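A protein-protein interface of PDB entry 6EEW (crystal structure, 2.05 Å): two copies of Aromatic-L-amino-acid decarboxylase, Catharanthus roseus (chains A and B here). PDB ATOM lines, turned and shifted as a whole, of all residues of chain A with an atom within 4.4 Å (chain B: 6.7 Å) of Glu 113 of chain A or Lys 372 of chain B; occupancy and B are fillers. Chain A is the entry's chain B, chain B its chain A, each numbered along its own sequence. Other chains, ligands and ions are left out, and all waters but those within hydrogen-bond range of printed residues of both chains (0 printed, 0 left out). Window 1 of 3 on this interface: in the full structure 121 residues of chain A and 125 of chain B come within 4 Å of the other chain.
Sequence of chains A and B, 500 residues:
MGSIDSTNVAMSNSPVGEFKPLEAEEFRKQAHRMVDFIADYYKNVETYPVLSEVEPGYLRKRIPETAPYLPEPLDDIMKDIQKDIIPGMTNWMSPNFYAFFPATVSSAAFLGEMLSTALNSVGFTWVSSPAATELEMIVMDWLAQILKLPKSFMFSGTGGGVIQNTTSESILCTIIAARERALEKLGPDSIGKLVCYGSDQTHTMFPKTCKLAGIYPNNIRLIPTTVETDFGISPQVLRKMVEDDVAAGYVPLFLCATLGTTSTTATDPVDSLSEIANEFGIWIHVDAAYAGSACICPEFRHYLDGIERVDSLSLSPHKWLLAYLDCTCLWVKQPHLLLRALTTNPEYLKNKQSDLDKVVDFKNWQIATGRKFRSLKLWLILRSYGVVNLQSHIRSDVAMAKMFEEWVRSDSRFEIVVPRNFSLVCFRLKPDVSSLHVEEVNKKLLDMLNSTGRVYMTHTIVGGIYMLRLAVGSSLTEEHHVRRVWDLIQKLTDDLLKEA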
ATOM      1  N   ALA A 109     -28.897  36.613 -36.120  1.00  0.00           N
ATOM      2  CA  ALA A 109     -28.179  35.396 -35.792  1.00  0.00           C
ATOM      3  C   ALA A 109     -28.758  34.738 -34.544  1.00  0.00           C
ATOM      4  O   ALA A 109     -28.832  33.508 -34.469  1.00  0.00           O
ATOM      5  CB  ALA A 109     -26.697  35.699 -35.602  1.00  0.00           C
ATOM      6  N   PHE A 110     -29.182  35.532 -33.553  1.00  0.00           N
ATOM      7  CA  PHE A 110     -29.767  34.926 -32.366  1.00  0.00           C
ATOM      8  C   PHE A 110     -31.058  34.193 -32.700  1.00  0.00           C
ATOM      9  O   PHE A 110     -31.326  33.121 -32.141  1.00  0.00           O
ATOM     10  CB  PHE A 110     -30.008  35.966 -31.268  1.00  0.00           C
ATOM     11  CG  PHE A 110     -30.320  35.345 -29.931  1.00  0.00           C
ATOM     12  CD1 PHE A 110     -29.308  34.788 -29.161  1.00  0.00           C
ATOM     13  CD2 PHE A 110     -31.624  35.281 -29.458  1.00  0.00           C
ATOM     14  CE1 PHE A 110     -29.588  34.188 -27.943  1.00  0.00           C
ATOM     15  CE2 PHE A 110     -31.915  34.685 -28.233  1.00  0.00           C
ATOM     16  CZ  PHE A 110     -30.898  34.137 -27.476  1.00  0.00           C
ATOM     17  N   LEU A 111     -31.878  34.749 -33.598  1.00  0.00           N
ATOM     18  CA  LEU A 111     -33.071  34.016 -34.011  1.00  0.00           C
ATOM     19  C   LEU A 111     -32.690  32.721 -34.698  1.00  0.00           C
ATOM     20  O   LEU A 111     -33.343  31.688 -34.499  1.00  0.00           O
ATOM     21  CB  LEU A 111     -33.963  34.842 -34.935  1.00  0.00           C
ATOM     22  CG  LEU A 111     -34.531  36.138 -34.376  1.00  0.00           C
ATOM     23  CD1 LEU A 111     -35.510  36.733 -35.387  1.00  0.00           C
ATOM     24  CD2 LEU A 111     -35.177  35.960 -33.033  1.00  0.00           C
ATOM     25  N   GLY A 112     -31.640  32.757 -35.520  1.00  0.00           N
ATOM     26  CA  GLY A 112     -31.194  31.526 -36.150  1.00  0.00           C
ATOM     27  C   GLY A 112     -30.750  30.483 -35.140  1.00  0.00           C
ATOM     28  O   GLY A 112     -31.063  29.299 -35.279  1.00  0.00           O
ATOM     29  N   GLU A 113     -30.018  30.914 -34.109  1.00  0.00           N
ATOM     30  CA  GLU A 113     -29.611  30.007 -33.037  1.00  0.00           C
ATOM     31  C   GLU A 113     -30.824  29.429 -32.308  1.00  0.00           C
ATOM     32  O   GLU A 113     -30.923  28.212 -32.097  1.00  0.00           O
ATOM     33  CB  GLU A 113     -28.678  30.733 -32.064  1.00  0.00           C
ATOM     34  CG  GLU A 113     -27.219  30.762 -32.518  1.00  0.00           C
ATOM     35  CD  GLU A 113     -26.495  29.438 -32.251  1.00  0.00           C
ATOM     36  OE1 GLU A 113     -27.043  28.589 -31.515  1.00  0.00           O
ATOM     37  OE2 GLU A 113     -25.387  29.229 -32.796  1.00  0.00           O
ATOM     38  N   MET A 114     -31.765  30.291 -31.922  1.00  0.00           N
ATOM     39  CA  MET A 114     -32.968  29.819 -31.246  1.00  0.00           C
ATOM     40  C   MET A 114     -33.678  28.751 -32.064  1.00  0.00           C
ATOM     41  O   MET A 114     -33.946  27.647 -31.578  1.00  0.00           O
ATOM     42  CB  MET A 114     -33.925  30.979 -30.992  1.00  0.00           C
ATOM     43  CG  MET A 114     -33.432  31.994 -29.988  1.00  0.00           C
ATOM     44  SD  MET A 114     -34.647  33.298 -29.701  1.00  0.00           S
ATOM     45  CE  MET A 114     -35.916  32.328 -28.892  1.00  0.00           C
ATOM     46  N   LEU A 115     -34.004  29.072 -33.316  1.00  0.00           N
ATOM     47  CA  LEU A 115     -34.797  28.144 -34.114  1.00  0.00           C
ATOM     48  C   LEU A 115     -34.028  26.865 -34.413  1.00  0.00           C
ATOM     49  O   LEU A 115     -34.585  25.762 -34.303  1.00  0.00           O
ATOM     50  CB  LEU A 115     -35.252  28.812 -35.403  1.00  0.00           C
ATOM     51  CG  LEU A 115     -36.159  27.992 -36.316  1.00  0.00           C
ATOM     52  CD1 LEU A 115     -37.382  27.463 -35.573  1.00  0.00           C
ATOM     53  CD2 LEU A 115     -36.568  28.834 -37.516  1.00  0.00           C
ATOM     54  N   SER A 116     -32.756  26.989 -34.796  1.00  0.00           N
ATOM     55  CA  SER A 116     -31.954  25.817 -35.110  1.00  0.00           C
ATOM     56  C   SER A 116     -31.864  24.884 -33.908  1.00  0.00           C
ATOM     57  O   SER A 116     -31.855  23.652 -34.059  1.00  0.00           O
ATOM     58  CB  SER A 116     -30.571  26.269 -35.573  1.00  0.00           C
ATOM     59  OG  SER A 116     -29.706  25.170 -35.721  1.00  0.00           O
ATOM     60  N   THR A 117     -31.763  25.450 -32.702  1.00  0.00           N
ATOM     61  CA  THR A 117     -31.735  24.611 -31.516  1.00  0.00           C
ATOM     62  C   THR A 117     -33.096  23.969 -31.288  1.00  0.00           C
ATOM     63  O   THR A 117     -33.203  22.745 -31.138  1.00  0.00           O
ATOM     64  CB  THR A 117     -31.309  25.434 -30.297  1.00  0.00           C
ATOM     65  OG1 THR A 117     -29.968  25.909 -30.476  1.00  0.00           O
ATOM     66  CG2 THR A 117     -31.367  24.588 -29.038  1.00  0.00           C
ATOM     67  N   LEU A 325     -20.885  32.299 -31.630  1.00  0.00           N
ATOM     68  CA  LEU A 325     -20.225  31.005 -31.553  1.00  0.00           C
ATOM     69  C   LEU A 325     -21.310  29.940 -31.577  1.00  0.00           C
ATOM     70  O   LEU A 325     -22.326  30.085 -30.904  1.00  0.00           O
ATOM     71  CB  LEU A 325     -19.402  30.905 -30.269  1.00  0.00           C
ATOM     72  CG  LEU A 325     -18.003  31.522 -30.336  1.00  0.00           C
ATOM     73  CD1 LEU A 325     -18.106  33.032 -30.379  1.00  0.00           C
ATOM     74  CD2 LEU A 325     -17.196  31.109 -29.120  1.00  0.00           C
ATOM     75  N   ASP A 326     -21.102  28.860 -32.327  1.00  0.00           N
ATOM     76  CA  ASP A 326     -19.950  28.633 -33.160  1.00  0.00           C
ATOM     77  C   ASP A 326     -20.304  28.857 -34.620  1.00  0.00           C
ATOM     78  O   ASP A 326     -21.442  28.627 -35.039  1.00  0.00           O
ATOM     79  CB  ASP A 326     -19.452  27.206 -32.968  1.00  0.00           C
ATOM     80  CG  ASP A 326     -18.974  26.948 -31.564  1.00  0.00           C
ATOM     81  OD1 ASP A 326     -18.172  27.762 -31.058  1.00  0.00           O
ATOM     82  OD2 ASP A 326     -19.406  25.930 -30.968  1.00  0.00           O
ATOM     83  N   LYS A 372     -25.619  20.145 -35.840  1.00  0.00           N
ATOM     84  CA  LYS A 372     -26.787  21.008 -35.781  1.00  0.00           C
ATOM     85  C   LYS A 372     -27.126  21.545 -37.176  1.00  0.00           C
ATOM     86  O   LYS A 372     -26.425  21.311 -38.174  1.00  0.00           O
ATOM     87  CB  LYS A 372     -26.550  22.177 -34.825  1.00  0.00           C
ATOM     88  CG  LYS A 372     -26.134  21.798 -33.428  1.00  0.00           C
ATOM     89  CD  LYS A 372     -26.062  23.005 -32.485  1.00  0.00           C
ATOM     90  CE  LYS A 372     -27.400  23.714 -32.383  1.00  0.00           C
ATOM     91  NZ  LYS A 372     -27.515  24.520 -31.140  1.00  0.00           N
ATOM     92  N   LYS A 377     -28.670  30.141 -39.308  1.00  0.00           N
ATOM     93  CA  LYS A 377     -28.415  31.491 -38.829  1.00  0.00           C
ATOM     94  C   LYS A 377     -27.608  32.302 -39.833  1.00  0.00           C
ATOM     95  O   LYS A 377     -27.807  33.515 -39.944  1.00  0.00           O
ATOM     96  CB  LYS A 377     -27.729  31.458 -37.469  1.00  0.00           C
ATOM     97  CG  LYS A 377     -26.320  30.911 -37.463  1.00  0.00           C
ATOM     98  CD  LYS A 377     -25.723  31.100 -36.068  1.00  0.00           C
ATOM     99  CE  LYS A 377     -24.407  30.349 -35.887  1.00  0.00           C
ATOM    100  NZ  LYS A 377     -23.853  30.655 -34.562  1.00  0.00           N
ATOM    101  N   ILE B  38     -41.600  29.101 -32.148  1.00  0.00           N
ATOM    102  CA  ILE B  38     -41.029  27.824 -31.730  1.00  0.00           C
ATOM    103  C   ILE B  38     -42.029  27.039 -30.894  1.00  0.00           C
ATOM    104  O   ILE B  38     -42.153  25.816 -31.033  1.00  0.00           O
ATOM    105  CB  ILE B  38     -39.721  28.055 -30.953  1.00  0.00           C
ATOM    106  CG1 ILE B  38     -38.632  28.635 -31.859  1.00  0.00           C
ATOM    107  CG2 ILE B  38     -39.268  26.760 -30.260  1.00  0.00           C
ATOM    108  CD1 ILE B  38     -37.324  28.958 -31.125  1.00  0.00           C
ATOM    109  N   PHE B 110     -33.216  24.578 -23.010  1.00  0.00           N
ATOM    110  CA  PHE B 110     -33.366  25.633 -24.002  1.00  0.00           C
ATOM    111  C   PHE B 110     -33.060  26.996 -23.405  1.00  0.00           C
ATOM    112  O   PHE B 110     -32.456  27.850 -24.067  1.00  0.00           O
ATOM    113  CB  PHE B 110     -34.768  25.623 -24.587  1.00  0.00           C
ATOM    114  CG  PHE B 110     -34.893  26.447 -25.815  1.00  0.00           C
ATOM    115  CD1 PHE B 110     -34.392  25.984 -27.023  1.00  0.00           C
ATOM    116  CD2 PHE B 110     -35.498  27.694 -25.771  1.00  0.00           C
ATOM    117  CE1 PHE B 110     -34.504  26.754 -28.179  1.00  0.00           C
ATOM    118  CE2 PHE B 110     -35.616  28.470 -26.922  1.00  0.00           C
ATOM    119  CZ  PHE B 110     -35.125  27.999 -28.124  1.00  0.00           C
ATOM    120  N   GLU B 113     -29.381  27.179 -23.382  1.00  0.00           N
ATOM    121  CA  GLU B 113     -28.875  27.484 -24.711  1.00  0.00           C
ATOM    122  C   GLU B 113     -29.023  28.967 -25.026  1.00  0.00           C
ATOM    123  O   GLU B 113     -28.063  29.618 -25.459  1.00  0.00           O
ATOM    124  CB  GLU B 113     -29.598  26.633 -25.750  1.00  0.00           C
ATOM    125  CG  GLU B 113     -29.004  25.239 -25.880  1.00  0.00           C
ATOM    126  CD  GLU B 113     -27.721  25.218 -26.729  1.00  0.00           C
ATOM    127  OE1 GLU B 113     -27.428  26.241 -27.396  1.00  0.00           O
ATOM    128  OE2 GLU B 113     -27.003  24.186 -26.728  1.00  0.00           O
ATOM    129  N   SER B 116     -26.599  30.950 -22.720  1.00  0.00           N
ATOM    130  CA  SER B 116     -25.218  30.661 -23.062  1.00  0.00           C
ATOM    131  C   SER B 116     -24.831  31.354 -24.354  1.00  0.00           C
ATOM    132  O   SER B 116     -23.717  31.882 -24.483  1.00  0.00           O
ATOM    133  CB  SER B 116     -25.038  29.149 -23.191  1.00  0.00           C
ATOM    134  OG  SER B 116     -23.773  28.838 -23.741  1.00  0.00           O
ATOM    135  N   THR B 117     -25.753  31.375 -25.320  1.00  0.00           N
ATOM    136  CA  THR B 117     -25.493  32.034 -26.583  1.00  0.00           C
ATOM    137  C   THR B 117     -25.464  33.548 -26.416  1.00  0.00           C
ATOM    138  O   THR B 117     -24.493  34.204 -26.801  1.00  0.00           O
ATOM    139  CB  THR B 117     -26.549  31.614 -27.593  1.00  0.00           C
ATOM    140  OG1 THR B 117     -26.449  30.200 -27.803  1.00  0.00           O
ATOM    141  CG2 THR B 117     -26.322  32.353 -28.901  1.00  0.00           C
ATOM    142  N   ALA B 118     -26.488  34.112 -25.782  1.00  0.00           N
ATOM    143  CA  ALA B 118     -26.558  35.557 -25.616  1.00  0.00           C
ATOM    144  C   ALA B 118     -25.305  36.099 -24.940  1.00  0.00           C
ATOM    145  O   ALA B 118     -24.795  37.155 -25.327  1.00  0.00           O
ATOM    146  CB  ALA B 118     -27.805  35.930 -24.818  1.00  0.00           C
ATOM    147  N   ASN B 120     -22.401  34.775 -25.079  1.00  0.00           N
ATOM    148  CA  ASN B 120     -21.444  34.660 -26.161  1.00  0.00           C
ATOM    149  C   ASN B 120     -20.031  34.868 -25.638  1.00  0.00           C
ATOM    150  O   ASN B 120     -19.237  35.623 -26.199  1.00  0.00           O
ATOM    151  CB  ASN B 120     -21.775  35.655 -27.285  1.00  0.00           C
ATOM    152  CG  ASN B 120     -21.111  35.299 -28.606  1.00  0.00           C
ATOM    153  OD1 ASN B 120     -21.043  34.128 -28.978  1.00  0.00           O
ATOM    154  ND2 ASN B 120     -20.628  36.317 -29.333  1.00  0.00           N
ATOM    155  N   SER B 121     -19.728  34.219 -24.521  1.00  0.00           N
ATOM    156  CA  SER B 121     -18.376  34.245 -23.990  1.00  0.00           C
ATOM    157  C   SER B 121     -17.550  33.155 -24.650  1.00  0.00           C
ATOM    158  O   SER B 121     -18.077  32.167 -25.156  1.00  0.00           O
ATOM    159  CB  SER B 121     -18.390  34.057 -22.481  1.00  0.00           C
ATOM    160  OG  SER B 121     -19.009  32.821 -22.175  1.00  0.00           O
ATOM    161  N   VAL B 122     -16.237  33.361 -24.662  1.00  0.00           N
ATOM    162  CA  VAL B 122     -15.295  32.425 -25.257  1.00  0.00           C
ATOM    163  C   VAL B 122     -14.420  31.944 -24.112  1.00  0.00           C
ATOM    164  O   VAL B 122     -13.542  32.680 -23.645  1.00  0.00           O
ATOM    165  CB  VAL B 122     -14.449  33.073 -26.360  1.00  0.00           C
ATOM    166  CG1 VAL B 122     -13.760  32.012 -27.155  1.00  0.00           C
ATOM    167  CG2 VAL B 122     -15.299  34.022 -27.265  1.00  0.00           C
ATOM    168  N   GLY B 123     -14.637  30.710 -23.667  1.00  0.00           N
ATOM    169  CA  GLY B 123     -14.025  30.285 -22.426  1.00  0.00           C
ATOM    170  C   GLY B 123     -12.771  29.464 -22.605  1.00  0.00           C
ATOM    171  O   GLY B 123     -12.659  28.386 -22.016  1.00  0.00           O
ATOM    172  N   ALA B 132     -17.692  30.533 -16.368  1.00  0.00           N
ATOM    173  CA  ALA B 132     -17.932  29.450 -17.322  1.00  0.00           C
ATOM    174  C   ALA B 132     -17.107  28.219 -16.968  1.00  0.00           C
ATOM    175  O   ALA B 132     -17.651  27.118 -16.803  1.00  0.00           O
ATOM    176  CB  ALA B 132     -17.629  29.907 -18.745  1.00  0.00           C
ATOM    177  N   GLU B 136     -18.328  24.672 -15.163  1.00  0.00           N
ATOM    178  CA  GLU B 136     -18.157  23.415 -15.884  1.00  0.00           C
ATOM    179  C   GLU B 136     -17.513  22.356 -15.004  1.00  0.00           C
ATOM    180  O   GLU B 136     -17.949  21.197 -14.984  1.00  0.00           O
ATOM    181  CB  GLU B 136     -17.334  23.633 -17.145  1.00  0.00           C
ATOM    182  CG  GLU B 136     -17.173  22.379 -17.995  1.00  0.00           C
ATOM    183  CD  GLU B 136     -16.971  22.697 -19.469  1.00  0.00           C
ATOM    184  OE1 GLU B 136     -17.345  23.823 -19.893  1.00  0.00           O
ATOM    185  OE2 GLU B 136     -16.483  21.807 -20.209  1.00  0.00           O
ATOM    186  N   ASN B 165     -18.258  18.557 -27.738  1.00  0.00           N
ATOM    187  CA  ASN B 165     -19.426  18.637 -28.607  1.00  0.00           C
ATOM    188  C   ASN B 165     -19.963  17.258 -28.964  1.00  0.00           C
ATOM    189  O   ASN B 165     -21.180  17.055 -29.005  1.00  0.00           O
ATOM    190  CB  ASN B 165     -19.064  19.376 -29.899  1.00  0.00           C
ATOM    191  CG  ASN B 165     -18.876  20.867 -29.693  1.00  0.00           C
ATOM    192  OD1 ASN B 165     -19.688  21.522 -29.053  1.00  0.00           O
ATOM    193  ND2 ASN B 165     -17.782  21.399 -30.209  1.00  0.00           N
ATOM    194  N   GLY B 370     -11.367  28.230 -28.904  1.00  0.00           N
ATOM    195  CA  GLY B 370     -12.620  28.790 -28.435  1.00  0.00           C
ATOM    196  C   GLY B 370     -13.625  27.726 -28.013  1.00  0.00           C
ATOM    197  O   GLY B 370     -13.595  26.584 -28.470  1.00  0.00           O
ATOM    198  N   ARG B 371     -14.566  28.153 -27.166  1.00  0.00           N
ATOM    199  CA  ARG B 371     -15.607  27.316 -26.577  1.00  0.00           C
ATOM    200  C   ARG B 371     -16.770  28.195 -26.157  1.00  0.00           C
ATOM    201  O   ARG B 371     -16.565  29.317 -25.688  1.00  0.00           O
ATOM    202  CB  ARG B 371     -15.126  26.546 -25.342  1.00  0.00           C
ATOM    203  CG  ARG B 371     -14.260  25.382 -25.586  1.00  0.00           C
ATOM    204  CD  ARG B 371     -13.559  24.993 -24.300  1.00  0.00           C
ATOM    205  NE  ARG B 371     -14.380  25.240 -23.130  1.00  0.00           N
ATOM    206  CZ  ARG B 371     -15.103  24.328 -22.485  1.00  0.00           C
ATOM    207  NH1 ARG B 371     -15.127  23.059 -22.871  1.00  0.00           N
ATOM    208  NH2 ARG B 371     -15.808  24.709 -21.438  1.00  0.00           N
ATOM    209  N   LYS B 372     -17.989  27.674 -26.309  1.00  0.00           N
ATOM    210  CA  LYS B 372     -19.148  28.325 -25.708  1.00  0.00           C
ATOM    211  C   LYS B 372     -19.201  28.069 -24.200  1.00  0.00           C
ATOM    212  O   LYS B 372     -18.372  27.357 -23.625  1.00  0.00           O
ATOM    213  CB  LYS B 372     -20.438  27.862 -26.380  1.00  0.00           C
ATOM    214  CG  LYS B 372     -20.429  28.099 -27.873  1.00  0.00           C
ATOM    215  CD  LYS B 372     -21.768  27.839 -28.538  1.00  0.00           C
ATOM    216  CE  LYS B 372     -22.848  28.709 -27.976  1.00  0.00           C
ATOM    217  NZ  LYS B 372     -24.004  28.836 -28.935  1.00  0.00           N
ATOM    218  N   PHE B 373     -20.193  28.689 -23.552  1.00  0.00           N
ATOM    219  CA  PHE B 373     -20.507  28.483 -22.140  1.00  0.00           C
ATOM    220  C   PHE B 373     -21.357  27.208 -22.004  1.00  0.00           C
ATOM    221  O   PHE B 373     -22.549  27.224 -21.691  1.00  0.00           O
ATOM    222  CB  PHE B 373     -21.205  29.727 -21.589  1.00  0.00           C
ATOM    223  CG  PHE B 373     -21.356  29.734 -20.101  1.00  0.00           C
ATOM    224  CD1 PHE B 373     -21.122  28.584 -19.360  1.00  0.00           C
ATOM    225  CD2 PHE B 373     -21.745  30.886 -19.441  1.00  0.00           C
ATOM    226  CE1 PHE B 373     -21.270  28.582 -17.995  1.00  0.00           C
ATOM    227  CE2 PHE B 373     -21.901  30.902 -18.073  1.00  0.00           C
ATOM    228  CZ  PHE B 373     -21.672  29.753 -17.344  1.00  0.00           C
ATOM    229  N   ARG B 374     -20.691  26.076 -22.222  1.00  0.00           N
ATOM    230  CA  ARG B 374     -21.381  24.816 -22.463  1.00  0.00           C
ATOM    231  C   ARG B 374     -22.090  24.280 -21.220  1.00  0.00           C
ATOM    232  O   ARG B 374     -23.124  23.614 -21.335  1.00  0.00           O
ATOM    233  CB  ARG B 374     -20.378  23.774 -22.976  1.00  0.00           C
ATOM    234  CG  ARG B 374     -19.772  24.036 -24.357  1.00  0.00           C
ATOM    235  CD  ARG B 374     -18.660  23.027 -24.710  1.00  0.00           C
ATOM    236  NE  ARG B 374     -18.104  23.308 -26.031  1.00  0.00           N
ATOM    237  CZ  ARG B 374     -16.981  22.783 -26.517  1.00  0.00           C
ATOM    238  NH1 ARG B 374     -16.267  21.932 -25.791  1.00  0.00           N
ATOM    239  NH2 ARG B 374     -16.565  23.109 -27.736  1.00  0.00           N
ATOM    240  N   SER B 375     -21.548  24.531 -20.029  1.00  0.00           N
ATOM    241  CA  SER B 375     -22.029  23.869 -18.823  1.00  0.00           C
ATOM    242  C   SER B 375     -23.322  24.472 -18.294  1.00  0.00           C
ATOM    243  O   SER B 375     -24.019  23.822 -17.495  1.00  0.00           O
ATOM    244  CB  SER B 375     -20.956  23.940 -17.736  1.00  0.00           C
ATOM    245  OG  SER B 375     -20.708  25.299 -17.371  1.00  0.00           O
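The backbone NH (N) of Leu 325 of chain A sits at hydrogen-bond distance from the side-chain amide oxygen (OD1) of Asn 120 of chain B.
OE1 of Glu 113 of chain A is in salt-bridge range of NZ of Lys 372 of chain B (3.99 Å).
The side-chain amino group of Lys 372 of chain B is in hydrogen-bond range of the backbone carbonyl oxygen of Leu 325 of chain A.
The backbone carbonyl oxygen of Glu 113 of chain B sits at hydrogen-bond distance from the side-chain hydroxyl of Thr 117 of chain B (2.9 Å).
OG1 of Thr 117 of chain B is in hydrogen-bond range of NZ of Lys 372 of chain B (3.0 Å).
The backbone NH (N) of Gly 123 of chain B lies within hydrogen-bond range of the backbone carbonyl oxygen (O) of Arg 371 of chain B, 3.1 Å away.
The guanidinium group (NH2) of Arg 371 of chain B is in salt-bridge range of the side-chain carboxylate (OE2) of Glu 136 of chain B (3.2 Å).
The backbone carbonyl oxygen (O) of Glu 113 of chain A is in hydrogen-bond range of the side-chain hydroxyl (OG1) of Thr 117 of chain A (3.0 Å).
The side-chain carboxylate (OE2) of Glu 113 of chain A lies within salt-bridge range of the side-chain amino group (NZ) of Lys 377 of chain A.
Among the printed residues, merely in contact across the chains: Met 114 of chain A with Phe 110 of chain B, Met 114 of chain A with Ile 38 of chain B, Phe 110 of chain A with Ala 118 of chain B, Phe 110 of chain A with Thr 117 of chain B, Asp 326 of chain A with Lys 372 of chain B, Thr 117 of chain A with Phe 110 of chain B, Leu 325 of chain A with Arg 371 of chain B, Leu 325 of chain A with Val 122 of chain B, Leu 115 of chain A with Ile 38 of chain B and Thr 117 of chain A with Glu 113 of chain B.
Printed residues of chain B within 4 Å of Glu 113 of chain A: Lys 372 (3.99 Å).
Printed residues of chain B within 4 Å of Thr 117 of chain A: Phe 110 and Glu 113.
Of the printed residues of chain A, Ile 38 of chain B touches Met 114 and Leu 115.
Of the printed residues of chain A, Phe 110 of chain B touches Met 114 (3.6 Å) and Thr 117 (3.9 Å).
Glu 136 of chain B touches none of the printed residues of chain A.
Asn 165 of chain B touches none of the printed residues of chain A.
Of the printed residues of chain A, Lys 372 of chain B touches Glu 113, Leu 325 and Asp 326.
The nearest printed residue of chain A that does not touch Lys 372 of chain B is Lys 377 of chain A (5.9 Å).
The nearest printed residue of chain A that does not touch Asn 120 of chain B is Asp 326 of chain A (6.2 Å).
Printed residues of chain A that touch a printed residue of chain B: Phe 110, Glu 113, Met 114, Leu 115, Thr 117, Leu 325 and Asp 326.
Along chain A the printed residues that touch a printed residue of chain B span positions 110 to 326.
Of the 19 printed residues of chain B, 9 touch a printed residue of chain A.
Printed residues of chain B that touch a printed residue of chain A: Ile 38, Phe 110, Glu 113, Thr 117, Ala 118, Asn 120, Val 122, Arg 371 and Lys 372.
Hydrophobic or aromatic side chains of chain B within 4 Å of the printed part of chain A: Ile 38, Phe 110, Ala 118 and Val 122.
Among the printed residues, Asp or Glu carboxylates within 4 Å of a Lys or Arg side-chain nitrogen of the other chain: Glu 113 of chain A with Lys 372 of chain B.
Phe 110 of chain A touches Thr 117 of chain B, and with the chains exchanged Thr 117 of chain A touches Phe 110 of chain B.
Glu 113 of chain A touches Lys 372 of chain B, but with the chains exchanged Lys 372 of chain A does not touch Glu 113 of chain B (4.1 Å).
Thr 117 of chain A touches Glu 113 of chain B, but with the chains exchanged Glu 113 of chain A does not touch Thr 117 of chain B (4.1 Å).
Of the 13 pairs that touch across the chains among the printed residues, 2 have their exchanged pair printed and touching as well.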
